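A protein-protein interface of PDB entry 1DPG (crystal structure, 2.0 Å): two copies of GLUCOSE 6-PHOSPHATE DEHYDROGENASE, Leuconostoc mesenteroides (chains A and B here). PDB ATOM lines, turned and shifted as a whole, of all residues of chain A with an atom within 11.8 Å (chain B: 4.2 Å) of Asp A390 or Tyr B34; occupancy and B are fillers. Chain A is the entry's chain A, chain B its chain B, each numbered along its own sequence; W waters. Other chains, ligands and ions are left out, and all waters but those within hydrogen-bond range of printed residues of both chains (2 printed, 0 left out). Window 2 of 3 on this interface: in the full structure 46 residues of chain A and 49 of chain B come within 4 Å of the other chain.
No position is printed for both chains. Of the 5 pairs that touch across the chains among the printed residues, none has its exchanged pair printed and touching as well.
Printed residues of chain B within 4 Å of Asp A390: Lys B32 (3.1 Å), Tyr B34 (2.6 Å), Pro B412 (3.9 Å) and His B420 (3.96 Å). Val B1 touches none of the printed residues of chain A. No residue of chain A comes within 4 Å of Ser B2. No residue of chain A comes within 4 Å of Glu B3. No residue of chain A comes within 4 Å of Ile B4. Leu B29 touches none of the printed residues of chain A. Of chain A, only Asp A390 (3.1 Å) comes within 4 Å of Lys B32. No residue of chain A comes within 4 Å of Gly B33. Tyr B34 touches just one residue of chain A: Asp A390 (2.6 Å). No residue of chain A comes within 4 Å of Leu B35. No residue of chain A comes within 4 Å of Gln B36. Printed residues of chain A within 4 Å of Pro B412: Asp A390. Of the printed residues of chain A, Arg B417 touches Glu A389. The nearest printed residue of chain B that does not touch Asp A390 is Arg B417 (4.01 Å). The nearest residue of chain A that does not touch Tyr B34 is Ala A391 (5.7 Å). The nearest printed residue of chain A that does not touch His B420 is Ala A391 (6.2 Å).
Hydrophobic or aromatic side chains of chain B within 4 Å of the printed part of chain A: Tyr B34, Pro B412 and His B420.
Among the printed residues, pairs that only touch across the chains: Asp A390 with Pro B412 and Asp A390 with His B420.
The backbone carbonyl oxygen (O) of Glu A389 sits at hydrogen-bond distance from the side-chain amino group (NZ) of Lys A386, at 3.4 Å. The side-chain hydroxyl (OG) of Ser A387 lies close to the side-chain carboxylate (OE1) of Glu A389. The side-chain carboxylate (OE1) of Glu A389 lies within hydrogen-bond range of the side-chain amide nitrogen (ND2) of Asn A393, at 2.9 Å. N of Ile B4 is in hydrogen-bond range of O of Tyr B34 (2.8 Å). N of Tyr B34 sits at hydrogen-bond distance from O of Leu B29, 2.9 Å away.
Water W1 bridges ND1 of His B420 (2.7 Å) and OD1 of Asp A390 (3.1 Å). Water W2 lies within hydrogen-bond range of O of Asp A390 (3.1 Å), NE of Arg B417 (3.4 Å) and ND1 of His B420 (3.5 Å).
The backbone carbonyl oxygen of Glu A389 is in hydrogen-bond range of the guanidinium group of Arg B417. The side-chain carboxylate (OD1) of Asp A390 lies within salt-bridge range of the side-chain amino group (NZ) of Lys B32 (3.1 Å). OH of Tyr B34 is in hydrogen-bond range of OD2 of Asp A390 (2.6 Å).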
ATOM      1  N   PHE A 358     -14.496   6.259 -16.033  1.00  0.00           N
ATOM      2  CA  PHE A 358     -13.524   7.255 -15.632  1.00  0.00           C
ATOM      3  C   PHE A 358     -13.496   7.348 -14.124  1.00  0.00           C
ATOM      4  O   PHE A 358     -12.624   7.999 -13.557  1.00  0.00           O
ATOM      5  CB  PHE A 358     -13.903   8.617 -16.213  1.00  0.00           C
ATOM      6  CG  PHE A 358     -13.750   8.695 -17.694  1.00  0.00           C
ATOM      7  CD1 PHE A 358     -14.763   8.249 -18.533  1.00  0.00           C
ATOM      8  CD2 PHE A 358     -12.574   9.184 -18.254  1.00  0.00           C
ATOM      9  CE1 PHE A 358     -14.603   8.282 -19.911  1.00  0.00           C
ATOM     10  CE2 PHE A 358     -12.402   9.223 -19.626  1.00  0.00           C
ATOM     11  CZ  PHE A 358     -13.417   8.772 -20.457  1.00  0.00           C
ATOM     12  N   GLY A 359     -14.479   6.717 -13.484  1.00  0.00           N
ATOM     13  CA  GLY A 359     -14.573   6.756 -12.040  1.00  0.00           C
ATOM     14  C   GLY A 359     -15.072   8.121 -11.611  1.00  0.00           C
ATOM     15  O   GLY A 359     -14.890   8.520 -10.462  1.00  0.00           O
ATOM     16  N   SER A 360     -15.663   8.855 -12.550  1.00  0.00           N
ATOM     17  CA  SER A 360     -16.192  10.182 -12.274  1.00  0.00           C
ATOM     18  C   SER A 360     -17.663  10.075 -11.871  1.00  0.00           C
ATOM     19  O   SER A 360     -18.283   9.015 -11.996  1.00  0.00           O
ATOM     20  CB  SER A 360     -16.036  11.086 -13.511  1.00  0.00           C
ATOM     21  OG  SER A 360     -16.574  10.464 -14.674  1.00  0.00           O
ATOM     22  N   GLU A 361     -18.216  11.182 -11.394  1.00  0.00           N
ATOM     23  CA  GLU A 361     -19.602  11.222 -10.982  1.00  0.00           C
ATOM     24  C   GLU A 361     -20.516  10.978 -12.191  1.00  0.00           C
ATOM     25  O   GLU A 361     -21.452  10.185 -12.125  1.00  0.00           O
ATOM     26  CB  GLU A 361     -19.900  12.573 -10.320  1.00  0.00           C
ATOM     27  CG  GLU A 361     -21.181  13.270 -10.809  1.00  0.00           C
ATOM     28  CD  GLU A 361     -21.986  13.894  -9.674  1.00  0.00           C
ATOM     29  OE1 GLU A 361     -21.548  14.942  -9.136  1.00  0.00           O
ATOM     30  OE2 GLU A 361     -23.054  13.329  -9.318  1.00  0.00           O
ATOM     31  N   LYS A 386     -14.383  16.613 -21.141  1.00  0.00           N
ATOM     32  CA  LYS A 386     -14.227  16.837 -19.703  1.00  0.00           C
ATOM     33  C   LYS A 386     -14.968  18.090 -19.224  1.00  0.00           C
ATOM     34  O   LYS A 386     -14.968  19.109 -19.914  1.00  0.00           O
ATOM     35  CB  LYS A 386     -12.742  16.973 -19.370  1.00  0.00           C
ATOM     36  CG  LYS A 386     -12.465  17.293 -17.923  1.00  0.00           C
ATOM     37  CD  LYS A 386     -11.000  17.600 -17.722  1.00  0.00           C
ATOM     38  CE  LYS A 386     -10.726  17.822 -16.255  1.00  0.00           C
ATOM     39  NZ  LYS A 386     -11.467  18.967 -15.684  1.00  0.00           N
ATOM     40  N   SER A 387     -15.610  18.010 -18.064  1.00  0.00           N
ATOM     41  CA  SER A 387     -16.305  19.156 -17.481  1.00  0.00           C
ATOM     42  C   SER A 387     -15.266  20.141 -17.012  1.00  0.00           C
ATOM     43  O   SER A 387     -14.105  19.787 -16.831  1.00  0.00           O
ATOM     44  CB  SER A 387     -17.047  18.754 -16.217  1.00  0.00           C
ATOM     45  OG  SER A 387     -17.819  17.600 -16.428  1.00  0.00           O
ATOM     46  N   VAL A 388     -15.694  21.374 -16.785  1.00  0.00           N
ATOM     47  CA  VAL A 388     -14.807  22.397 -16.259  1.00  0.00           C
ATOM     48  C   VAL A 388     -15.095  22.427 -14.747  1.00  0.00           C
ATOM     49  O   VAL A 388     -15.895  23.235 -14.272  1.00  0.00           O
ATOM     50  CB  VAL A 388     -15.064  23.763 -16.924  1.00  0.00           C
ATOM     51  CG1 VAL A 388     -14.153  24.824 -16.347  1.00  0.00           C
ATOM     52  CG2 VAL A 388     -14.801  23.651 -18.401  1.00  0.00           C
ATOM     53  N   GLU A 389     -14.539  21.437 -14.041  1.00  0.00           N
ATOM     54  CA  GLU A 389     -14.676  21.263 -12.588  1.00  0.00           C
ATOM     55  C   GLU A 389     -13.316  20.867 -11.995  1.00  0.00           C
ATOM     56  O   GLU A 389     -12.403  20.446 -12.718  1.00  0.00           O
ATOM     57  CB  GLU A 389     -15.670  20.151 -12.258  1.00  0.00           C
ATOM     58  CG  GLU A 389     -17.109  20.402 -12.641  1.00  0.00           C
ATOM     59  CD  GLU A 389     -17.956  19.156 -12.453  1.00  0.00           C
ATOM     60  OE1 GLU A 389     -17.995  18.325 -13.379  1.00  0.00           O
ATOM     61  OE2 GLU A 389     -18.547  18.982 -11.368  1.00  0.00           O
ATOM     62  N   ASP A 390     -13.204  20.939 -10.672  1.00  0.00           N
ATOM     63  CA  ASP A 390     -11.945  20.616 -10.004  1.00  0.00           C
ATOM     64  C   ASP A 390     -11.595  19.138 -10.033  1.00  0.00           C
ATOM     65  O   ASP A 390     -10.419  18.770 -10.059  1.00  0.00           O
ATOM     66  CB  ASP A 390     -11.951  21.157  -8.578  1.00  0.00           C
ATOM     67  CG  ASP A 390     -12.268  22.638  -8.528  1.00  0.00           C
ATOM     68  OD1 ASP A 390     -11.551  23.427  -9.188  1.00  0.00           O
ATOM     69  OD2 ASP A 390     -13.247  23.010  -7.846  1.00  0.00           O
ATOM     70  N   ALA A 391     -12.614  18.292 -10.018  1.00  0.00           N
ATOM     71  CA  ALA A 391     -12.405  16.852 -10.081  1.00  0.00           C
ATOM     72  C   ALA A 391     -12.793  16.410 -11.493  1.00  0.00           C
ATOM     73  O   ALA A 391     -13.757  16.930 -12.069  1.00  0.00           O
ATOM     74  CB  ALA A 391     -13.268  16.151  -9.053  1.00  0.00           C
ATOM     75  N   PHE A 392     -12.036  15.470 -12.050  1.00  0.00           N
ATOM     76  CA  PHE A 392     -12.300  14.973 -13.390  1.00  0.00           C
ATOM     77  C   PHE A 392     -13.730  14.479 -13.492  1.00  0.00           C
ATOM     78  O   PHE A 392     -14.189  13.669 -12.686  1.00  0.00           O
ATOM     79  CB  PHE A 392     -11.341  13.836 -13.754  1.00  0.00           C
ATOM     80  CG  PHE A 392     -11.402  13.442 -15.204  1.00  0.00           C
ATOM     81  CD1 PHE A 392     -12.404  12.581 -15.668  1.00  0.00           C
ATOM     82  CD2 PHE A 392     -10.483  13.959 -16.115  1.00  0.00           C
ATOM     83  CE1 PHE A 392     -12.495  12.244 -17.020  1.00  0.00           C
ATOM     84  CE2 PHE A 392     -10.563  13.631 -17.467  1.00  0.00           C
ATOM     85  CZ  PHE A 392     -11.578  12.767 -17.920  1.00  0.00           C
ATOM     86  N   ASN A 393     -14.422  14.935 -14.521  1.00  0.00           N
ATOM     87  CA  ASN A 393     -15.797  14.532 -14.715  1.00  0.00           C
ATOM     88  C   ASN A 393     -16.152  14.743 -16.183  1.00  0.00           C
ATOM     89  O   ASN A 393     -15.526  15.570 -16.862  1.00  0.00           O
ATOM     90  CB  ASN A 393     -16.693  15.373 -13.812  1.00  0.00           C
ATOM     91  CG  ASN A 393     -18.048  14.771 -13.639  1.00  0.00           C
ATOM     92  OD1 ASN A 393     -18.208  13.554 -13.719  1.00  0.00           O
ATOM     93  ND2 ASN A 393     -19.037  15.604 -13.369  1.00  0.00           N
ATOM     94  N   THR A 394     -17.096  13.968 -16.705  1.00  0.00           N
ATOM     95  CA  THR A 394     -17.451  14.139 -18.106  1.00  0.00           C
ATOM     96  C   THR A 394     -18.664  15.036 -18.300  1.00  0.00           C
ATOM     97  O   THR A 394     -19.492  15.196 -17.399  1.00  0.00           O
ATOM     98  CB  THR A 394     -17.694  12.792 -18.829  1.00  0.00           C
ATOM     99  OG1 THR A 394     -18.875  12.158 -18.320  1.00  0.00           O
ATOM    100  CG2 THR A 394     -16.501  11.872 -18.662  1.00  0.00           C
ATOM    101  N   ARG A 395     -18.745  15.641 -19.479  1.00  0.00           N
ATOM    102  CA  ARG A 395     -19.853  16.509 -19.842  1.00  0.00           C
ATOM    103  C   ARG A 395     -20.076  16.245 -21.334  1.00  0.00           C
ATOM    104  O   ARG A 395     -19.268  15.586 -21.993  1.00  0.00           O
ATOM    105  CB  ARG A 395     -19.483  17.982 -19.644  1.00  0.00           C
ATOM    106  CG  ARG A 395     -18.862  18.577 -20.886  1.00  0.00           C
ATOM    107  CD  ARG A 395     -17.857  19.623 -20.610  1.00  0.00           C
ATOM    108  NE  ARG A 395     -18.481  20.920 -20.472  1.00  0.00           N
ATOM    109  CZ  ARG A 395     -17.871  22.061 -20.761  1.00  0.00           C
ATOM    110  NH1 ARG A 395     -16.624  22.064 -21.217  1.00  0.00           N
ATOM    111  NH2 ARG A 395     -18.489  23.205 -20.529  1.00  0.00           N
ATOM    112  N   VAL B   1     -17.899  21.453  -0.923  1.00  0.00           N
ATOM    113  CA  VAL B   1     -16.414  21.308  -0.883  1.00  0.00           C
ATOM    114  C   VAL B   1     -15.998  20.890   0.520  1.00  0.00           C
ATOM    115  O   VAL B   1     -16.652  21.251   1.495  1.00  0.00           O
ATOM    116  CB  VAL B   1     -15.686  22.639  -1.254  1.00  0.00           C
ATOM    117  CG1 VAL B   1     -15.971  23.013  -2.700  1.00  0.00           C
ATOM    118  CG2 VAL B   1     -16.118  23.773  -0.320  1.00  0.00           C
ATOM    119  N   SER B   2     -14.942  20.094   0.610  1.00  0.00           N
ATOM    120  CA  SER B   2     -14.436  19.633   1.896  1.00  0.00           C
ATOM    121  C   SER B   2     -13.141  20.387   2.173  1.00  0.00           C
ATOM    122  O   SER B   2     -12.380  20.685   1.248  1.00  0.00           O
ATOM    123  CB  SER B   2     -14.155  18.130   1.846  1.00  0.00           C
ATOM    124  OG  SER B   2     -15.271  17.421   1.335  1.00  0.00           O
ATOM    125  N   GLU B   3     -12.914  20.726   3.439  1.00  0.00           N
ATOM    126  CA  GLU B   3     -11.709  21.442   3.833  1.00  0.00           C
ATOM    127  C   GLU B   3     -10.522  20.509   3.685  1.00  0.00           C
ATOM    128  O   GLU B   3     -10.596  19.337   4.071  1.00  0.00           O
ATOM    129  CB  GLU B   3     -11.807  21.901   5.288  1.00  0.00           C
ATOM    130  CG  GLU B   3     -10.633  22.747   5.732  1.00  0.00           C
ATOM    131  CD  GLU B   3     -10.632  23.013   7.218  1.00  0.00           C
ATOM    132  OE1 GLU B   3     -11.510  23.770   7.688  1.00  0.00           O
ATOM    133  OE2 GLU B   3      -9.755  22.459   7.915  1.00  0.00           O
ATOM    134  N   ILE B   4      -9.452  21.015   3.085  1.00  0.00           N
ATOM    135  CA  ILE B   4      -8.232  20.238   2.898  1.00  0.00           C
ATOM    136  C   ILE B   4      -7.298  20.673   4.019  1.00  0.00           C
ATOM    137  O   ILE B   4      -7.151  21.871   4.282  1.00  0.00           O
ATOM    138  CB  ILE B   4      -7.562  20.520   1.512  1.00  0.00           C
ATOM    139  CG1 ILE B   4      -8.516  20.142   0.369  1.00  0.00           C
ATOM    140  CG2 ILE B   4      -6.236  19.751   1.390  1.00  0.00           C
ATOM    141  CD1 ILE B   4      -7.993  20.480  -1.005  1.00  0.00           C
ATOM    142  N   LEU B  29      -7.631  28.431  -4.343  1.00  0.00           N
ATOM    143  CA  LEU B  29      -8.018  27.231  -3.601  1.00  0.00           C
ATOM    144  C   LEU B  29      -8.693  27.621  -2.284  1.00  0.00           C
ATOM    145  O   LEU B  29      -9.554  26.903  -1.764  1.00  0.00           O
ATOM    146  CB  LEU B  29      -6.779  26.385  -3.319  1.00  0.00           C
ATOM    147  CG  LEU B  29      -6.756  24.978  -3.904  1.00  0.00           C
ATOM    148  CD1 LEU B  29      -7.032  25.012  -5.398  1.00  0.00           C
ATOM    149  CD2 LEU B  29      -5.403  24.339  -3.608  1.00  0.00           C
ATOM    150  N   LYS B  32     -12.291  29.309  -3.184  1.00  0.00           N
ATOM    151  CA  LYS B  32     -13.232  28.255  -3.553  1.00  0.00           C
ATOM    152  C   LYS B  32     -13.651  27.407  -2.347  1.00  0.00           C
ATOM    153  O   LYS B  32     -14.470  26.492  -2.482  1.00  0.00           O
ATOM    154  CB  LYS B  32     -12.638  27.352  -4.637  1.00  0.00           C
ATOM    155  CG  LYS B  32     -12.478  28.001  -6.000  1.00  0.00           C
ATOM    156  CD  LYS B  32     -11.900  26.986  -6.970  1.00  0.00           C
ATOM    157  CE  LYS B  32     -11.821  27.548  -8.367  1.00  0.00           C
ATOM    158  NZ  LYS B  32     -11.429  26.494  -9.336  1.00  0.00           N
ATOM    159  N   GLY B  33     -13.039  27.668  -1.193  1.00  0.00           N
ATOM    160  CA  GLY B  33     -13.385  26.942   0.015  1.00  0.00           C
ATOM    161  C   GLY B  33     -12.623  25.676   0.346  1.00  0.00           C
ATOM    162  O   GLY B  33     -12.935  25.032   1.344  1.00  0.00           O
ATOM    163  N   TYR B  34     -11.635  25.297  -0.455  1.00  0.00           N
ATOM    164  CA  TYR B  34     -10.871  24.086  -0.150  1.00  0.00           C
ATOM    165  C   TYR B  34      -9.952  24.347   1.041  1.00  0.00           C
ATOM    166  O   TYR B  34      -9.776  23.490   1.912  1.00  0.00           O
ATOM    167  CB  TYR B  34     -10.057  23.632  -1.361  1.00  0.00           C
ATOM    168  CG  TYR B  34     -10.908  23.105  -2.489  1.00  0.00           C
ATOM    169  CD1 TYR B  34     -11.461  21.823  -2.429  1.00  0.00           C
ATOM    170  CD2 TYR B  34     -11.188  23.899  -3.602  1.00  0.00           C
ATOM    171  CE1 TYR B  34     -12.278  21.347  -3.447  1.00  0.00           C
ATOM    172  CE2 TYR B  34     -12.005  23.434  -4.627  1.00  0.00           C
ATOM    173  CZ  TYR B  34     -12.550  22.159  -4.544  1.00  0.00           C
ATOM    174  OH  TYR B  34     -13.379  21.707  -5.547  1.00  0.00           O
ATOM    175  N   LEU B  35      -9.377  25.544   1.066  1.00  0.00           N
ATOM    176  CA  LEU B  35      -8.487  25.967   2.136  1.00  0.00           C
ATOM    177  C   LEU B  35      -9.327  26.804   3.088  1.00  0.00           C
ATOM    178  O   LEU B  35      -9.692  27.929   2.760  1.00  0.00           O
ATOM    179  CB  LEU B  35      -7.346  26.808   1.550  1.00  0.00           C
ATOM    180  CG  LEU B  35      -5.959  26.173   1.400  1.00  0.00           C
ATOM    181  CD1 LEU B  35      -6.045  24.675   1.186  1.00  0.00           C
ATOM    182  CD2 LEU B  35      -5.213  26.859   0.272  1.00  0.00           C
ATOM    183  N   GLN B  36      -9.681  26.238   4.237  1.00  0.00           N
ATOM    184  CA  GLN B  36     -10.494  26.957   5.206  1.00  0.00           C
ATOM    185  C   GLN B  36      -9.755  27.488   6.427  1.00  0.00           C
ATOM    186  O   GLN B  36      -9.545  28.695   6.549  1.00  0.00           O
ATOM    187  CB  GLN B  36     -11.654  26.092   5.664  1.00  0.00           C
ATOM    188  CG  GLN B  36     -12.662  25.777   4.593  1.00  0.00           C
ATOM    189  CD  GLN B  36     -13.630  24.702   5.040  1.00  0.00           C
ATOM    190  OE1 GLN B  36     -13.979  24.607   6.221  1.00  0.00           O
ATOM    191  NE2 GLN B  36     -14.031  23.854   4.110  1.00  0.00           N
ATOM    192  N   PRO B 412      -9.597  26.252 -13.920  1.00  0.00           N
ATOM    193  CA  PRO B 412      -8.494  26.489 -12.987  1.00  0.00           C
ATOM    194  C   PRO B 412      -7.225  26.810 -13.777  1.00  0.00           C
ATOM    195  O   PRO B 412      -7.104  26.442 -14.950  1.00  0.00           O
ATOM    196  CB  PRO B 412      -8.351  25.133 -12.287  1.00  0.00           C
ATOM    197  CG  PRO B 412      -9.724  24.504 -12.422  1.00  0.00           C
ATOM    198  CD  PRO B 412     -10.083  24.863 -13.827  1.00  0.00           C
ATOM    199  N   ARG B 417      -4.461  23.691 -10.514  1.00  0.00           N
ATOM    200  CA  ARG B 417      -4.844  22.330 -10.823  1.00  0.00           C
ATOM    201  C   ARG B 417      -3.812  21.361 -10.253  1.00  0.00           C
ATOM    202  O   ARG B 417      -4.152  20.395  -9.573  1.00  0.00           O
ATOM    203  CB  ARG B 417      -4.962  22.174 -12.345  1.00  0.00           C
ATOM    204  CG  ARG B 417      -4.984  20.749 -12.866  1.00  0.00           C
ATOM    205  CD  ARG B 417      -6.012  19.847 -12.160  1.00  0.00           C
ATOM    206  NE  ARG B 417      -7.396  20.324 -12.194  1.00  0.00           N
ATOM    207  CZ  ARG B 417      -7.999  20.867 -13.251  1.00  0.00           C
ATOM    208  NH1 ARG B 417      -7.354  21.037 -14.408  1.00  0.00           N
ATOM    209  NH2 ARG B 417      -9.283  21.194 -13.170  1.00  0.00           N
ATOM    210  N   HIS B 420      -3.624  21.437  -6.299  1.00  0.00           N
ATOM    211  CA  HIS B 420      -4.811  20.771  -5.808  1.00  0.00           C
ATOM    212  C   HIS B 420      -4.641  19.265  -5.952  1.00  0.00           C
ATOM    213  O   HIS B 420      -4.847  18.511  -4.999  1.00  0.00           O
ATOM    214  CB  HIS B 420      -6.029  21.233  -6.589  1.00  0.00           C
ATOM    215  CG  HIS B 420      -7.327  20.878  -5.940  1.00  0.00           C
ATOM    216  ND1 HIS B 420      -8.506  21.538  -6.222  1.00  0.00           N
ATOM    217  CD2 HIS B 420      -7.632  19.944  -5.004  1.00  0.00           C
ATOM    218  CE1 HIS B 420      -9.475  21.033  -5.489  1.00  0.00           C
ATOM    219  NE2 HIS B 420      -8.978  20.066  -4.741  1.00  0.00           N
HETATM  220  O   HOH W   1      -8.653  23.460  -8.134  1.00  0.00           O
HETATM  221  O   HOH W   2      -7.598  19.470  -8.889  1.00  0.00           O
